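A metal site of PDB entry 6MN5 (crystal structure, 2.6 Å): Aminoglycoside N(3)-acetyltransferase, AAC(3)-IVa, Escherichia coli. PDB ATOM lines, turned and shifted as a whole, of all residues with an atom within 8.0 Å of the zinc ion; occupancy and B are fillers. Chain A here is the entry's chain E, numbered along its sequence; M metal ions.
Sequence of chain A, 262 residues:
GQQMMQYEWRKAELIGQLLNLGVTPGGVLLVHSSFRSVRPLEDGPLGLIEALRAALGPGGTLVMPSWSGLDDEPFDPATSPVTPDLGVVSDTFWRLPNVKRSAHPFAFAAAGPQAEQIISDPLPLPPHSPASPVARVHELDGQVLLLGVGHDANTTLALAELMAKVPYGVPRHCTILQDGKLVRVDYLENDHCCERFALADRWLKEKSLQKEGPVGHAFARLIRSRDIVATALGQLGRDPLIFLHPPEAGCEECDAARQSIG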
ATOM      1  N   HIS A 192     -12.925 -31.290   3.867  1.00  0.00           N
ATOM      2  CA  HIS A 192     -13.299 -29.918   3.593  1.00  0.00           C
ATOM      3  C   HIS A 192     -12.661 -29.517   2.269  1.00  0.00           C
ATOM      4  O   HIS A 192     -12.292 -30.386   1.481  1.00  0.00           O
ATOM      5  CB  HIS A 192     -12.882 -28.976   4.731  1.00  0.00           C
ATOM      6  CG  HIS A 192     -11.629 -29.409   5.439  1.00  0.00           C
ATOM      7  ND1 HIS A 192     -10.374 -29.024   5.025  1.00  0.00           N
ATOM      8  CD2 HIS A 192     -11.443 -30.196   6.529  1.00  0.00           C
ATOM      9  CE1 HIS A 192      -9.466 -29.552   5.831  1.00  0.00           C
ATOM     10  NE2 HIS A 192     -10.089 -30.261   6.751  1.00  0.00           N
ATOM     11  N   CYS A 193     -12.522 -28.224   2.016  1.00  0.00           N
ATOM     12  CA  CYS A 193     -11.811 -27.783   0.822  1.00  0.00           C
ATOM     13  C   CYS A 193     -10.301 -27.935   0.957  1.00  0.00           C
ATOM     14  O   CYS A 193      -9.597 -27.865  -0.061  1.00  0.00           O
ATOM     15  CB  CYS A 193     -12.140 -26.328   0.512  1.00  0.00           C
ATOM     16  SG  CYS A 193     -11.680 -25.207   1.835  1.00  0.00           S
ATOM     17  N   CYS A 194      -9.792 -28.126   2.167  1.00  0.00           N
ATOM     18  CA  CYS A 194      -8.377 -28.331   2.455  1.00  0.00           C
ATOM     19  C   CYS A 194      -7.492 -27.180   1.981  1.00  0.00           C
ATOM     20  O   CYS A 194      -6.277 -27.350   1.898  1.00  0.00           O
ATOM     21  CB  CYS A 194      -7.853 -29.663   1.892  1.00  0.00           C
ATOM     22  SG  CYS A 194      -9.007 -31.045   1.947  1.00  0.00           S
ATOM     23  N   GLU A 195      -8.064 -26.017   1.675  1.00  0.00           N
ATOM     24  CA  GLU A 195      -7.255 -24.878   1.276  1.00  0.00           C
ATOM     25  C   GLU A 195      -6.280 -24.482   2.376  1.00  0.00           C
ATOM     26  O   GLU A 195      -5.173 -24.010   2.085  1.00  0.00           O
ATOM     27  CB  GLU A 195      -8.138 -23.679   0.913  1.00  0.00           C
ATOM     28  CG  GLU A 195      -8.501 -23.561  -0.560  1.00  0.00           C
ATOM     29  CD  GLU A 195      -9.874 -22.926  -0.762  1.00  0.00           C
ATOM     30  OE1 GLU A 195     -10.457 -22.418   0.219  1.00  0.00           O
ATOM     31  OE2 GLU A 195     -10.375 -22.955  -1.907  1.00  0.00           O
ATOM     32  N   ARG A 196      -6.676 -24.654   3.632  1.00  0.00           N
ATOM     33  CA  ARG A 196      -5.892 -24.195   4.775  1.00  0.00           C
ATOM     34  C   ARG A 196      -4.866 -25.231   5.243  1.00  0.00           C
ATOM     35  O   ARG A 196      -4.265 -25.036   6.306  1.00  0.00           O
ATOM     36  CB  ARG A 196      -6.814 -23.826   5.933  1.00  0.00           C
ATOM     37  N   PHE A 243      -8.029 -26.137  10.824  1.00  0.00           N
ATOM     38  CA  PHE A 243      -7.997 -26.357   9.388  1.00  0.00           C
ATOM     39  C   PHE A 243      -9.253 -25.887   8.677  1.00  0.00           C
ATOM     40  O   PHE A 243      -9.389 -26.125   7.462  1.00  0.00           O
ATOM     41  CB  PHE A 243      -7.754 -27.835   9.088  1.00  0.00           C
ATOM     42  CG  PHE A 243      -6.361 -28.294   9.407  1.00  0.00           C
ATOM     43  CD1 PHE A 243      -6.120 -29.588   9.833  1.00  0.00           C
ATOM     44  CD2 PHE A 243      -5.291 -27.426   9.277  1.00  0.00           C
ATOM     45  CE1 PHE A 243      -4.835 -30.003  10.118  1.00  0.00           C
ATOM     46  CE2 PHE A 243      -4.006 -27.840   9.562  1.00  0.00           C
ATOM     47  CZ  PHE A 243      -3.776 -29.127   9.990  1.00  0.00           C
ATOM     48  N   LEU A 244     -10.172 -25.221   9.372  1.00  0.00           N
ATOM     49  CA  LEU A 244     -11.430 -24.823   8.774  1.00  0.00           C
ATOM     50  C   LEU A 244     -11.521 -23.303   8.637  1.00  0.00           C
ATOM     51  O   LEU A 244     -11.236 -22.569   9.581  1.00  0.00           O
ATOM     52  CB  LEU A 244     -12.641 -25.305   9.579  1.00  0.00           C
ATOM     53  CG  LEU A 244     -13.824 -25.356   8.614  1.00  0.00           C
ATOM     54  CD1 LEU A 244     -13.330 -25.894   7.285  1.00  0.00           C
ATOM     55  CD2 LEU A 244     -14.965 -26.207   9.142  1.00  0.00           C
ATOM     56  N   HIS A 245     -11.969 -22.859   7.465  1.00  0.00           N
ATOM     57  CA  HIS A 245     -12.106 -21.444   7.196  1.00  0.00           C
ATOM     58  C   HIS A 245     -13.271 -20.858   7.983  1.00  0.00           C
ATOM     59  O   HIS A 245     -14.320 -21.494   8.112  1.00  0.00           O
ATOM     60  CB  HIS A 245     -12.322 -21.211   5.698  1.00  0.00           C
ATOM     61  CG  HIS A 245     -11.091 -21.454   4.882  1.00  0.00           C
ATOM     62  ND1 HIS A 245     -10.723 -22.703   4.452  1.00  0.00           N
ATOM     63  CD2 HIS A 245     -10.129 -20.598   4.448  1.00  0.00           C
ATOM     64  CE1 HIS A 245      -9.586 -22.616   3.770  1.00  0.00           C
ATOM     65  NE2 HIS A 245      -9.211 -21.351   3.750  1.00  0.00           N
ATOM     66  N   PRO A 246     -13.125 -19.637   8.494  1.00  0.00           N
ATOM     67  CA  PRO A 246     -14.193 -19.030   9.312  1.00  0.00           C
ATOM     68  C   PRO A 246     -15.459 -18.820   8.500  1.00  0.00           C
ATOM     69  O   PRO A 246     -15.407 -18.745   7.258  1.00  0.00           O
ATOM     70  CB  PRO A 246     -13.571 -17.685   9.730  1.00  0.00           C
ATOM     71  CG  PRO A 246     -12.503 -17.412   8.713  1.00  0.00           C
ATOM     72  CD  PRO A 246     -11.955 -18.767   8.355  1.00  0.00           C
ATOM     73  N   ALA A 249     -15.374 -16.226   5.618  1.00  0.00           N
ATOM     74  CA  ALA A 249     -14.883 -16.599   4.300  1.00  0.00           C
ATOM     75  C   ALA A 249     -15.968 -17.212   3.430  1.00  0.00           C
ATOM     76  O   ALA A 249     -15.851 -17.169   2.197  1.00  0.00           O
ATOM     77  CB  ALA A 249     -13.713 -17.575   4.443  1.00  0.00           C
ATOM     78  N   GLY A 250     -17.007 -17.782   4.030  1.00  0.00           N
ATOM     79  CA  GLY A 250     -18.152 -18.272   3.280  1.00  0.00           C
ATOM     80  C   GLY A 250     -17.862 -19.445   2.368  1.00  0.00           C
ATOM     81  O   GLY A 250     -18.343 -19.469   1.233  1.00  0.00           O
ATOM     82  N   CYS A 251     -17.106 -20.425   2.848  1.00  0.00           N
ATOM     83  CA  CYS A 251     -16.834 -21.629   2.063  1.00  0.00           C
ATOM     84  C   CYS A 251     -17.815 -22.724   2.460  1.00  0.00           C
ATOM     85  O   CYS A 251     -17.994 -23.011   3.645  1.00  0.00           O
ATOM     86  CB  CYS A 251     -15.392 -22.087   2.255  1.00  0.00           C
ATOM     87  SG  CYS A 251     -15.005 -23.599   1.332  1.00  0.00           S
ATOM     88  N   GLU A 252     -18.445 -23.328   1.461  1.00  0.00           N
ATOM     89  CA  GLU A 252     -19.511 -24.302   1.720  1.00  0.00           C
ATOM     90  C   GLU A 252     -18.939 -25.650   2.159  1.00  0.00           C
ATOM     91  O   GLU A 252     -19.397 -26.223   3.150  1.00  0.00           O
ATOM     92  CB  GLU A 252     -20.392 -24.467   0.482  1.00  0.00           C
ATOM     93  CG  GLU A 252     -19.661 -24.287  -0.836  1.00  0.00           C
ATOM     94  CD  GLU A 252     -20.526 -24.670  -2.019  1.00  0.00           C
ATOM     95  OE1 GLU A 252     -21.465 -25.474  -1.827  1.00  0.00           O
ATOM     96  OE2 GLU A 252     -20.265 -24.180  -3.142  1.00  0.00           O
ATOM     97  N   GLU A 253     -17.957 -26.175   1.420  1.00  0.00           N
ATOM     98  CA  GLU A 253     -17.252 -27.377   1.858  1.00  0.00           C
ATOM     99  C   GLU A 253     -16.667 -27.190   3.245  1.00  0.00           C
ATOM    100  O   GLU A 253     -16.382 -28.184   3.934  1.00  0.00           O
ATOM    101  CB  GLU A 253     -16.142 -27.725   0.875  1.00  0.00           C
ATOM    102  CG  GLU A 253     -15.806 -29.197   0.817  1.00  0.00           C
ATOM    103  CD  GLU A 253     -15.413 -29.646  -0.575  1.00  0.00           C
ATOM    104  OE1 GLU A 253     -15.385 -30.864  -0.833  1.00  0.00           O
ATOM    105  OE2 GLU A 253     -15.132 -28.761  -1.414  1.00  0.00           O
ATOM    106  N   CYS A 254     -16.465 -25.945   3.659  1.00  0.00           N
ATOM    107  CA  CYS A 254     -15.985 -25.636   4.997  1.00  0.00           C
ATOM    108  C   CYS A 254     -17.115 -25.736   6.022  1.00  0.00           C
ATOM    109  O   CYS A 254     -17.125 -26.636   6.860  1.00  0.00           O
ATOM    110  CB  CYS A 254     -15.369 -24.243   5.015  1.00  0.00           C
ATOM    111  SG  CYS A 254     -13.702 -24.206   4.357  1.00  0.00           S
ATOM    112  N   ASP A 255     -18.101 -24.829   5.925  1.00  0.00           N
ATOM    113  CA  ASP A 255     -19.160 -24.761   6.919  1.00  0.00           C
ATOM    114  C   ASP A 255     -20.026 -26.015   6.988  1.00  0.00           C
ATOM    115  O   ASP A 255     -20.783 -26.170   7.939  1.00  0.00           O
ATOM    116  CB  ASP A 255     -20.041 -23.540   6.640  1.00  0.00           C
ATOM    117  CG  ASP A 255     -19.415 -22.254   7.151  1.00  0.00           C
ATOM    118  OD1 ASP A 255     -18.167 -22.224   7.287  1.00  0.00           O
ATOM    119  OD2 ASP A 255     -20.165 -21.292   7.420  1.00  0.00           O
HETATM  120 ZN    ZN M   1     -12.861 -23.473   3.042  1.00  0.00          ZN
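The side-chain sulfur (SG) of Cys 193 lies close to the side-chain carboxylate (OE1) of Glu 195 (3.4 Å). SG of Cys 193 lies close to ND1 of His 245 (3.7 Å). SG of Cys 254 lies close to ND1 of His 245, 3.3 Å away.
The zinc ion is bound by the side-chain sulfur of Cys 254 (1.7 Å), the side-chain sulfur of Cys 193 (2.4 Å) and the side-chain sulfur of Cys 251 (2.7 Å). The zinc ion has three donor atoms within binding distance. Slightly farther from the zinc ion lies a ring nitrogen (ND1) of His 245 (2.7 Å).
Glu 195 touches the zinc ion. Within 4 Å of the zinc ion: Cys 193, Glu 195, His 245, Cys 251 and Cys 254.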
